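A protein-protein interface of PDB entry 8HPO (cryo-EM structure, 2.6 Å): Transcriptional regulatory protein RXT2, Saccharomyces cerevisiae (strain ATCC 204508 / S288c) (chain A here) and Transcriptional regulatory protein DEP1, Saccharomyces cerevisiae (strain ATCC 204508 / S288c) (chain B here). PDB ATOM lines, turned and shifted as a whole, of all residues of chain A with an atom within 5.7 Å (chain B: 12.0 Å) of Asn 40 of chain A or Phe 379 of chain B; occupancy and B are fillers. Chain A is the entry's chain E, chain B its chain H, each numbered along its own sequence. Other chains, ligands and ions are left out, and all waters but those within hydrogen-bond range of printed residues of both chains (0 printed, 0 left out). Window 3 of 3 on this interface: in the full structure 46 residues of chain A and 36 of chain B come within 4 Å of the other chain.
The side-chain hydroxyl (OG) of Ser 38 of chain A lies within hydrogen-bond range of the side-chain amide nitrogen (ND2) of Asn 40 of chain A (3.4 Å).
The side-chain hydroxyl (OG) of Ser 381 of chain B lies within hydrogen-bond range of the backbone carbonyl oxygen (O) of Phe 379 of chain B (3.1 Å).
Of the 16 printed residues of chain B, 7 touch a printed residue of chain A.
Hydrophobic or aromatic side chains of chain B within 4 Å of the printed part of chain A: Leu 375 and Phe 379.
O of Phe 379 of chain B lies within hydrogen-bond range of OG1 of Thr 103 of chain A (3.5 Å).
OG1 of Thr 103 of chain A sits close to O of His 380 of chain B (3.2 Å).
OG of Ser 381 of chain B is in hydrogen-bond range of OG1 of Thr 103 of chain A (2.9 Å).
Among the printed residues, pairs that only touch across the chains: Leu 100 of chain A with Leu 375 of chain B (3.5 Å), Leu 100 of chain A with Phe 382 of chain B (3.6 Å), Val 91 of chain A with Phe 379 of chain B (3.6 Å), Leu 100 of chain A with Ser 381 of chain B (3.6 Å), Tyr 93 of chain A with Asp 371 of chain B (3.6 Å), Tyr 93 of chain A with Phe 379 of chain B (3.7 Å), Tyr 93 of chain A with Gly 374 of chain B (3.8 Å) and Asn 40 of chain A with Phe 379 of chain B (3.9 Å).
Phe 379 of chain B touches just these residues of chain A: Asn 40 (3.9 Å), Val 91 (3.6 Å), Tyr 93 (3.7 Å) and Thr 103 (3.5 Å).
No residue of chain B comes within 4 Å of Glu 36 of chain A.
No residue of chain B comes within 4 Å of Ser 38 of chain A.
No residue of chain B comes within 4 Å of Gln 42 of chain A.
Val 91 of chain A touches just one residue of chain B: Phe 379.
Tyr 93 of chain A touches just these residues of chain B: Asp 371 (3.6 Å), Gly 374 (3.8 Å) and Phe 379 (3.7 Å).
Thr 103 of chain A touches just these residues of chain B: Phe 379, His 380 and Ser 381.
Printed residues of chain A within 4 Å of Phe 382 of chain B: Leu 100.
Of the printed residues of chain A, His 380 of chain B touches Thr 103 (2.7 Å).
Phe 92 of chain A touches none of the printed residues of chain B.
Glu 373 of chain B touches none of the printed residues of chain A.
The nearest residue of chain B that does not touch Asn 40 of chain A is Tyr 378 of chain B (8.9 Å).
The nearest residue of chain A that does not touch Phe 379 of chain B is Phe 92 of chain A (4.2 Å).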
ATOM      1  N   LYS A  35      -6.063  16.498 -19.886  1.00  0.00           N
ATOM      2  CA  LYS A  35      -6.551  15.314 -20.580  1.00  0.00           C
ATOM      3  C   LYS A  35      -5.494  14.221 -20.644  1.00  0.00           C
ATOM      4  O   LYS A  35      -5.809  13.053 -20.404  1.00  0.00           O
ATOM      5  CB  LYS A  35      -7.024  15.680 -21.984  1.00  0.00           C
ATOM      6  CG  LYS A  35      -8.404  16.298 -22.030  1.00  0.00           C
ATOM      7  CD  LYS A  35      -9.090  15.957 -23.332  1.00  0.00           C
ATOM      8  CE  LYS A  35     -10.552  16.349 -23.312  1.00  0.00           C
ATOM      9  NZ  LYS A  35     -11.229  16.009 -24.589  1.00  0.00           N
ATOM     10  N   GLU A  36      -4.244  14.564 -20.956  1.00  0.00           N
ATOM     11  CA  GLU A  36      -3.213  13.534 -20.982  1.00  0.00           C
ATOM     12  C   GLU A  36      -2.840  13.066 -19.581  1.00  0.00           C
ATOM     13  O   GLU A  36      -2.208  12.015 -19.434  1.00  0.00           O
ATOM     14  CB  GLU A  36      -1.976  14.036 -21.728  1.00  0.00           C
ATOM     15  CG  GLU A  36      -1.044  12.930 -22.230  1.00  0.00           C
ATOM     16  CD  GLU A  36      -1.203  12.630 -23.717  1.00  0.00           C
ATOM     17  OE1 GLU A  36      -0.237  12.135 -24.333  1.00  0.00           O
ATOM     18  OE2 GLU A  36      -2.295  12.875 -24.270  1.00  0.00           O
ATOM     19  N   LYS A  37      -3.215  13.815 -18.546  1.00  0.00           N
ATOM     20  CA  LYS A  37      -3.045  13.355 -17.175  1.00  0.00           C
ATOM     21  C   LYS A  37      -4.293  12.685 -16.615  1.00  0.00           C
ATOM     22  O   LYS A  37      -4.279  12.248 -15.462  1.00  0.00           O
ATOM     23  CB  LYS A  37      -2.641  14.518 -16.265  1.00  0.00           C
ATOM     24  CG  LYS A  37      -1.156  14.821 -16.261  1.00  0.00           C
ATOM     25  CD  LYS A  37      -0.802  15.714 -15.089  1.00  0.00           C
ATOM     26  CE  LYS A  37      -1.278  15.104 -13.782  1.00  0.00           C
ATOM     27  NZ  LYS A  37      -0.943  15.958 -12.614  1.00  0.00           N
ATOM     28  N   SER A  38      -5.371  12.609 -17.397  1.00  0.00           N
ATOM     29  CA  SER A  38      -6.554  11.877 -16.956  1.00  0.00           C
ATOM     30  C   SER A  38      -6.270  10.398 -16.748  1.00  0.00           C
ATOM     31  O   SER A  38      -6.995   9.741 -15.996  1.00  0.00           O
ATOM     32  CB  SER A  38      -7.687  12.042 -17.965  1.00  0.00           C
ATOM     33  OG  SER A  38      -8.594  10.962 -17.873  1.00  0.00           O
ATOM     34  N   GLY A  39      -5.242   9.863 -17.398  1.00  0.00           N
ATOM     35  CA  GLY A  39      -4.895   8.466 -17.290  1.00  0.00           C
ATOM     36  C   GLY A  39      -5.300   7.619 -18.474  1.00  0.00           C
ATOM     37  O   GLY A  39      -4.882   6.461 -18.556  1.00  0.00           O
ATOM     38  N   ASN A  40      -6.102   8.154 -19.380  1.00  0.00           N
ATOM     39  CA  ASN A  40      -6.534   7.467 -20.585  1.00  0.00           C
ATOM     40  C   ASN A  40      -5.715   7.898 -21.802  1.00  0.00           C
ATOM     41  O   ASN A  40      -4.664   8.537 -21.719  1.00  0.00           O
ATOM     42  CB  ASN A  40      -8.023   7.715 -20.854  1.00  0.00           C
ATOM     43  CG  ASN A  40      -8.864   7.651 -19.602  1.00  0.00           C
ATOM     44  OD1 ASN A  40      -8.510   6.974 -18.642  1.00  0.00           O
ATOM     45  ND2 ASN A  40      -9.993   8.346 -19.608  1.00  0.00           N
ATOM     46  N   TYR A  41      -6.240   7.476 -22.939  1.00  0.00           N
ATOM     47  CA  TYR A  41      -6.035   7.885 -24.324  1.00  0.00           C
ATOM     48  C   TYR A  41      -4.816   7.398 -25.097  1.00  0.00           C
ATOM     49  O   TYR A  41      -4.970   7.180 -26.304  1.00  0.00           O
ATOM     50  CB  TYR A  41      -5.948   9.418 -24.393  1.00  0.00           C
ATOM     51  CG  TYR A  41      -7.134  10.174 -23.866  1.00  0.00           C
ATOM     52  CD1 TYR A  41      -8.299  10.276 -24.604  1.00  0.00           C
ATOM     53  CD2 TYR A  41      -7.084  10.797 -22.635  1.00  0.00           C
ATOM     54  CE1 TYR A  41      -9.383  10.967 -24.123  1.00  0.00           C
ATOM     55  CE2 TYR A  41      -8.161  11.489 -22.147  1.00  0.00           C
ATOM     56  CZ  TYR A  41      -9.309  11.571 -22.893  1.00  0.00           C
ATOM     57  OH  TYR A  41     -10.389  12.262 -22.407  1.00  0.00           O
ATOM     58  N   GLN A  42      -3.615   7.284 -24.513  1.00  0.00           N
ATOM     59  CA  GLN A  42      -2.614   6.257 -24.816  1.00  0.00           C
ATOM     60  C   GLN A  42      -1.239   6.906 -24.786  1.00  0.00           C
ATOM     61  O   GLN A  42      -1.096   8.061 -24.374  1.00  0.00           O
ATOM     62  CB  GLN A  42      -2.811   5.488 -26.115  1.00  0.00           C
ATOM     63  CG  GLN A  42      -3.130   4.032 -25.814  1.00  0.00           C
ATOM     64  CD  GLN A  42      -2.169   3.428 -24.793  1.00  0.00           C
ATOM     65  OE1 GLN A  42      -0.953   3.595 -24.887  1.00  0.00           O
ATOM     66  NE2 GLN A  42      -2.717   2.729 -23.805  1.00  0.00           N
ATOM     67  N   THR A  90      -8.860  -0.151 -20.976  1.00  0.00           N
ATOM     68  CA  THR A  90      -9.875   0.273 -20.023  1.00  0.00           C
ATOM     69  C   THR A  90      -9.910   1.797 -19.982  1.00  0.00           C
ATOM     70  O   THR A  90      -8.936   2.451 -20.358  1.00  0.00           O
ATOM     71  CB  THR A  90      -9.571  -0.298 -18.635  1.00  0.00           C
ATOM     72  OG1 THR A  90      -9.365  -1.712 -18.735  1.00  0.00           O
ATOM     73  CG2 THR A  90     -10.728  -0.064 -17.694  1.00  0.00           C
ATOM     74  N   VAL A  91     -11.025   2.355 -19.525  1.00  0.00           N
ATOM     75  CA  VAL A  91     -11.245   3.793 -19.522  1.00  0.00           C
ATOM     76  C   VAL A  91     -12.168   4.148 -18.365  1.00  0.00           C
ATOM     77  O   VAL A  91     -13.211   3.515 -18.182  1.00  0.00           O
ATOM     78  CB  VAL A  91     -11.826   4.265 -20.866  1.00  0.00           C
ATOM     79  CG1 VAL A  91     -12.789   5.406 -20.672  1.00  0.00           C
ATOM     80  CG2 VAL A  91     -10.710   4.678 -21.795  1.00  0.00           C
ATOM     81  N   PHE A  92     -11.785   5.151 -17.585  1.00  0.00           N
ATOM     82  CA  PHE A  92     -12.623   5.667 -16.510  1.00  0.00           C
ATOM     83  C   PHE A  92     -13.579   6.691 -17.106  1.00  0.00           C
ATOM     84  O   PHE A  92     -13.153   7.585 -17.840  1.00  0.00           O
ATOM     85  CB  PHE A  92     -11.764   6.284 -15.412  1.00  0.00           C
ATOM     86  CG  PHE A  92     -12.495   6.512 -14.126  1.00  0.00           C
ATOM     87  CD1 PHE A  92     -13.304   7.621 -13.962  1.00  0.00           C
ATOM     88  CD2 PHE A  92     -12.377   5.617 -13.082  1.00  0.00           C
ATOM     89  CE1 PHE A  92     -13.980   7.831 -12.786  1.00  0.00           C
ATOM     90  CE2 PHE A  92     -13.048   5.822 -11.906  1.00  0.00           C
ATOM     91  CZ  PHE A  92     -13.853   6.932 -11.757  1.00  0.00           C
ATOM     92  N   TYR A  93     -14.865   6.570 -16.794  1.00  0.00           N
ATOM     93  CA  TYR A  93     -15.875   7.453 -17.361  1.00  0.00           C
ATOM     94  C   TYR A  93     -17.144   7.417 -16.523  1.00  0.00           C
ATOM     95  O   TYR A  93     -17.671   6.341 -16.231  1.00  0.00           O
ATOM     96  CB  TYR A  93     -16.188   7.055 -18.802  1.00  0.00           C
ATOM     97  CG  TYR A  93     -17.391   7.740 -19.401  1.00  0.00           C
ATOM     98  CD1 TYR A  93     -18.518   7.020 -19.743  1.00  0.00           C
ATOM     99  CD2 TYR A  93     -17.389   9.098 -19.646  1.00  0.00           C
ATOM    100  CE1 TYR A  93     -19.612   7.634 -20.296  1.00  0.00           C
ATOM    101  CE2 TYR A  93     -18.483   9.721 -20.202  1.00  0.00           C
ATOM    102  CZ  TYR A  93     -19.590   8.981 -20.526  1.00  0.00           C
ATOM    103  OH  TYR A  93     -20.686   9.591 -21.079  1.00  0.00           O
ATOM    104  N   GLU A  97     -14.774   2.001 -14.341  1.00  0.00           N
ATOM    105  CA  GLU A  97     -13.947   1.566 -15.454  1.00  0.00           C
ATOM    106  C   GLU A  97     -14.758   0.735 -16.440  1.00  0.00           C
ATOM    107  O   GLU A  97     -15.467  -0.198 -16.058  1.00  0.00           O
ATOM    108  CB  GLU A  97     -12.755   0.760 -14.944  1.00  0.00           C
ATOM    109  CG  GLU A  97     -11.846   1.520 -13.986  1.00  0.00           C
ATOM    110  CD  GLU A  97     -10.657   2.173 -14.677  1.00  0.00           C
ATOM    111  OE1 GLU A  97     -10.639   3.415 -14.801  1.00  0.00           O
ATOM    112  OE2 GLU A  97      -9.730   1.445 -15.082  1.00  0.00           O
ATOM    113  N   LEU A 100     -13.148  -1.595 -23.679  1.00  0.00           N
ATOM    114  CA  LEU A 100     -13.414  -1.285 -25.074  1.00  0.00           C
ATOM    115  C   LEU A 100     -12.999  -2.456 -25.956  1.00  0.00           C
ATOM    116  O   LEU A 100     -11.991  -3.119 -25.715  1.00  0.00           O
ATOM    117  CB  LEU A 100     -12.665  -0.019 -25.493  1.00  0.00           C
ATOM    118  CG  LEU A 100     -12.660   1.135 -24.493  1.00  0.00           C
ATOM    119  CD1 LEU A 100     -11.552   2.107 -24.828  1.00  0.00           C
ATOM    120  CD2 LEU A 100     -13.987   1.840 -24.490  1.00  0.00           C
ATOM    121  N   THR A 103     -11.298   0.390 -30.305  1.00  0.00           N
ATOM    122  CA  THR A 103     -11.592   1.819 -30.298  1.00  0.00           C
ATOM    123  C   THR A 103     -11.691   2.488 -31.675  1.00  0.00           C
ATOM    124  O   THR A 103     -12.800   2.645 -32.188  1.00  0.00           O
ATOM    125  CB  THR A 103     -10.550   2.528 -29.414  1.00  0.00           C
ATOM    126  OG1 THR A 103     -10.760   3.945 -29.437  1.00  0.00           O
ATOM    127  CG2 THR A 103      -9.111   2.169 -29.801  1.00  0.00           C
ATOM    128  N   ILE B 369     -28.000   2.971 -21.243  1.00  0.00           N
ATOM    129  CA  ILE B 369     -27.900   3.117 -22.692  1.00  0.00           C
ATOM    130  C   ILE B 369     -27.204   4.425 -23.047  1.00  0.00           C
ATOM    131  O   ILE B 369     -26.354   4.476 -23.949  1.00  0.00           O
ATOM    132  CB  ILE B 369     -29.303   3.017 -23.316  1.00  0.00           C
ATOM    133  CG1 ILE B 369     -29.653   1.560 -23.602  1.00  0.00           C
ATOM    134  CG2 ILE B 369     -29.411   3.850 -24.571  1.00  0.00           C
ATOM    135  CD1 ILE B 369     -31.036   1.377 -24.140  1.00  0.00           C
ATOM    136  N   SER B 370     -27.548   5.501 -22.336  1.00  0.00           N
ATOM    137  CA  SER B 370     -26.903   6.785 -22.574  1.00  0.00           C
ATOM    138  C   SER B 370     -25.421   6.730 -22.240  1.00  0.00           C
ATOM    139  O   SER B 370     -24.602   7.331 -22.941  1.00  0.00           O
ATOM    140  CB  SER B 370     -27.588   7.879 -21.767  1.00  0.00           C
ATOM    141  OG  SER B 370     -26.651   8.845 -21.347  1.00  0.00           O
ATOM    142  N   ASP B 371     -25.050   6.017 -21.176  1.00  0.00           N
ATOM    143  CA  ASP B 371     -23.628   5.871 -20.869  1.00  0.00           C
ATOM    144  C   ASP B 371     -22.891   5.146 -21.987  1.00  0.00           C
ATOM    145  O   ASP B 371     -21.766   5.519 -22.341  1.00  0.00           O
ATOM    146  CB  ASP B 371     -23.436   5.138 -19.546  1.00  0.00           C
ATOM    147  CG  ASP B 371     -23.405   6.076 -18.354  1.00  0.00           C
ATOM    148  OD1 ASP B 371     -24.450   6.679 -18.031  1.00  0.00           O
ATOM    149  OD2 ASP B 371     -22.327   6.210 -17.739  1.00  0.00           O
ATOM    150  N   LEU B 372     -23.511   4.118 -22.568  1.00  0.00           N
ATOM    151  CA  LEU B 372     -22.860   3.416 -23.679  1.00  0.00           C
ATOM    152  C   LEU B 372     -22.688   4.322 -24.896  1.00  0.00           C
ATOM    153  O   LEU B 372     -21.597   4.397 -25.487  1.00  0.00           O
ATOM    154  CB  LEU B 372     -23.659   2.174 -24.054  1.00  0.00           C
ATOM    155  CG  LEU B 372     -23.636   1.047 -23.030  1.00  0.00           C
ATOM    156  CD1 LEU B 372     -24.550  -0.071 -23.468  1.00  0.00           C
ATOM    157  CD2 LEU B 372     -22.219   0.549 -22.838  1.00  0.00           C
ATOM    158  N   GLU B 373     -23.747   5.034 -25.280  1.00  0.00           N
ATOM    159  CA  GLU B 373     -23.648   5.880 -26.465  1.00  0.00           C
ATOM    160  C   GLU B 373     -22.715   7.058 -26.215  1.00  0.00           C
ATOM    161  O   GLU B 373     -22.103   7.592 -27.145  1.00  0.00           O
ATOM    162  CB  GLU B 373     -25.033   6.358 -26.901  1.00  0.00           C
ATOM    163  CG  GLU B 373     -25.649   7.423 -26.037  1.00  0.00           C
ATOM    164  CD  GLU B 373     -26.593   8.308 -26.820  1.00  0.00           C
ATOM    165  OE1 GLU B 373     -26.392   8.443 -28.043  1.00  0.00           O
ATOM    166  OE2 GLU B 373     -27.540   8.857 -26.222  1.00  0.00           O
ATOM    167  N   GLY B 374     -22.556   7.455 -24.955  1.00  0.00           N
ATOM    168  CA  GLY B 374     -21.600   8.501 -24.649  1.00  0.00           C
ATOM    169  C   GLY B 374     -20.172   8.013 -24.740  1.00  0.00           C
ATOM    170  O   GLY B 374     -19.293   8.727 -25.226  1.00  0.00           O
ATOM    171  N   LEU B 375     -19.916   6.806 -24.243  1.00  0.00           N
ATOM    172  CA  LEU B 375     -18.631   6.167 -24.487  1.00  0.00           C
ATOM    173  C   LEU B 375     -18.310   6.177 -25.972  1.00  0.00           C
ATOM    174  O   LEU B 375     -17.165   6.415 -26.373  1.00  0.00           O
ATOM    175  CB  LEU B 375     -18.658   4.741 -23.932  1.00  0.00           C
ATOM    176  CG  LEU B 375     -17.413   3.858 -23.898  1.00  0.00           C
ATOM    177  CD1 LEU B 375     -17.631   2.744 -22.914  1.00  0.00           C
ATOM    178  CD2 LEU B 375     -17.132   3.272 -25.258  1.00  0.00           C
ATOM    179  N   ARG B 376     -19.329   5.961 -26.809  1.00  0.00           N
ATOM    180  CA  ARG B 376     -19.093   5.980 -28.252  1.00  0.00           C
ATOM    181  C   ARG B 376     -18.791   7.383 -28.765  1.00  0.00           C
ATOM    182  O   ARG B 376     -17.846   7.574 -29.536  1.00  0.00           O
ATOM    183  CB  ARG B 376     -20.288   5.411 -29.006  1.00  0.00           C
ATOM    184  CG  ARG B 376     -19.964   5.083 -30.451  1.00  0.00           C
ATOM    185  CD  ARG B 376     -21.147   5.344 -31.358  1.00  0.00           C
ATOM    186  NE  ARG B 376     -21.381   6.771 -31.540  1.00  0.00           N
ATOM    187  CZ  ARG B 376     -22.553   7.365 -31.361  1.00  0.00           C
ATOM    188  NH1 ARG B 376     -23.608   6.655 -31.000  1.00  0.00           N
ATOM    189  NH2 ARG B 376     -22.671   8.670 -31.548  1.00  0.00           N
ATOM    190  N   LYS B 377     -19.589   8.376 -28.374  1.00  0.00           N
ATOM    191  CA  LYS B 377     -19.454   9.701 -28.973  1.00  0.00           C
ATOM    192  C   LYS B 377     -18.242  10.449 -28.425  1.00  0.00           C
ATOM    193  O   LYS B 377     -17.817  11.457 -28.995  1.00  0.00           O
ATOM    194  CB  LYS B 377     -20.724  10.522 -28.757  1.00  0.00           C
ATOM    195  CG  LYS B 377     -20.724  11.318 -27.471  1.00  0.00           C
ATOM    196  CD  LYS B 377     -21.955  12.196 -27.334  1.00  0.00           C
ATOM    197  CE  LYS B 377     -22.204  13.028 -28.579  1.00  0.00           C
ATOM    198  NZ  LYS B 377     -20.989  13.755 -29.032  1.00  0.00           N
ATOM    199  N   TYR B 378     -17.680   9.988 -27.305  1.00  0.00           N
ATOM    200  CA  TYR B 378     -16.529  10.677 -26.734  1.00  0.00           C
ATOM    201  C   TYR B 378     -15.222   9.916 -26.861  1.00  0.00           C
ATOM    202  O   TYR B 378     -14.199  10.536 -27.164  1.00  0.00           O
ATOM    203  CB  TYR B 378     -16.775  11.008 -25.264  1.00  0.00           C
ATOM    204  CG  TYR B 378     -17.697  12.176 -25.097  1.00  0.00           C
ATOM    205  CD1 TYR B 378     -17.482  13.342 -25.806  1.00  0.00           C
ATOM    206  CD2 TYR B 378     -18.783  12.118 -24.245  1.00  0.00           C
ATOM    207  CE1 TYR B 378     -18.320  14.417 -25.672  1.00  0.00           C
ATOM    208  CE2 TYR B 378     -19.626  13.194 -24.103  1.00  0.00           C
ATOM    209  CZ  TYR B 378     -19.387  14.340 -24.820  1.00  0.00           C
ATOM    210  OH  TYR B 378     -20.223  15.419 -24.688  1.00  0.00           O
ATOM    211  N   PHE B 379     -15.199   8.608 -26.626  1.00  0.00           N
ATOM    212  CA  PHE B 379     -13.963   7.861 -26.787  1.00  0.00           C
ATOM    213  C   PHE B 379     -13.908   7.122 -28.110  1.00  0.00           C
ATOM    214  O   PHE B 379     -12.924   6.422 -28.370  1.00  0.00           O
ATOM    215  CB  PHE B 379     -13.759   6.881 -25.624  1.00  0.00           C
ATOM    216  CG  PHE B 379     -13.817   7.528 -24.268  1.00  0.00           C
ATOM    217  CD1 PHE B 379     -12.668   7.963 -23.646  1.00  0.00           C
ATOM    218  CD2 PHE B 379     -15.025   7.693 -23.616  1.00  0.00           C
ATOM    219  CE1 PHE B 379     -12.723   8.555 -22.410  1.00  0.00           C
ATOM    220  CE2 PHE B 379     -15.083   8.285 -22.381  1.00  0.00           C
ATOM    221  CZ  PHE B 379     -13.932   8.713 -21.775  1.00  0.00           C
ATOM    222  N   HIS B 380     -14.928   7.274 -28.953  1.00  0.00           N
ATOM    223  CA  HIS B 380     -14.963   6.680 -30.286  1.00  0.00           C
ATOM    224  C   HIS B 380     -14.620   5.199 -30.226  1.00  0.00           C
ATOM    225  O   HIS B 380     -13.606   4.749 -30.759  1.00  0.00           O
ATOM    226  CB  HIS B 380     -14.024   7.424 -31.236  1.00  0.00           C
ATOM    227  CG  HIS B 380     -14.076   8.913 -31.089  1.00  0.00           C
ATOM    228  ND1 HIS B 380     -15.177   9.658 -31.450  1.00  0.00           N
ATOM    229  CD2 HIS B 380     -13.163   9.795 -30.616  1.00  0.00           C
ATOM    230  CE1 HIS B 380     -14.942  10.934 -31.204  1.00  0.00           C
ATOM    231  NE2 HIS B 380     -13.728  11.044 -30.696  1.00  0.00           N
ATOM    232  N   SER B 381     -15.471   4.434 -29.547  1.00  0.00           N
ATOM    233  CA  SER B 381     -15.175   3.042 -29.257  1.00  0.00           C
ATOM    234  C   SER B 381     -16.460   2.231 -29.265  1.00  0.00           C
ATOM    235  O   SER B 381     -17.568   2.772 -29.317  1.00  0.00           O
ATOM    236  CB  SER B 381     -14.480   2.902 -27.904  1.00  0.00           C
ATOM    237  OG  SER B 381     -13.135   3.320 -27.975  1.00  0.00           O
ATOM    238  N   PHE B 382     -16.295   0.918 -29.196  1.00  0.00           N
ATOM    239  CA  PHE B 382     -17.385  -0.020 -29.054  1.00  0.00           C
ATOM    240  C   PHE B 382     -17.367  -0.590 -27.647  1.00  0.00           C
ATOM    241  O   PHE B 382     -16.307  -1.036 -27.189  1.00  0.00           O
ATOM    242  CB  PHE B 382     -17.264  -1.147 -30.079  1.00  0.00           C
ATOM    243  CG  PHE B 382     -18.552  -1.837 -30.358  1.00  0.00           C
ATOM    244  CD1 PHE B 382     -18.759  -3.138 -29.953  1.00  0.00           C
ATOM    245  CD2 PHE B 382     -19.567  -1.177 -31.012  1.00  0.00           C
ATOM    246  CE1 PHE B 382     -19.949  -3.763 -30.200  1.00  0.00           C
ATOM    247  CE2 PHE B 382     -20.757  -1.798 -31.263  1.00  0.00           C
ATOM    248  CZ  PHE B 382     -20.951  -3.093 -30.859  1.00  0.00           C
ATOM    249  N   PRO B 383     -18.491  -0.575 -26.931  1.00  0.00           N
ATOM    250  CA  PRO B 383     -18.505  -1.080 -25.556  1.00  0.00           C
ATOM    251  C   PRO B 383     -17.983  -2.506 -25.446  1.00  0.00           C
ATOM    252  O   PRO B 383     -17.866  -3.230 -26.433  1.00  0.00           O
ATOM    253  CB  PRO B 383     -19.984  -0.988 -25.166  1.00  0.00           C
ATOM    254  CG  PRO B 383     -20.707  -0.518 -26.377  1.00  0.00           C
ATOM    255  CD  PRO B 383     -19.718   0.167 -27.230  1.00  0.00           C
ATOM    256  N   GLY B 384     -17.669  -2.905 -24.218  1.00  0.00           N
ATOM    257  CA  GLY B 384     -16.986  -4.157 -23.977  1.00  0.00           C
ATOM    258  C   GLY B 384     -17.613  -5.102 -22.972  1.00  0.00           C
ATOM    259  O   GLY B 384     -16.891  -5.633 -22.123  1.00  0.00           O
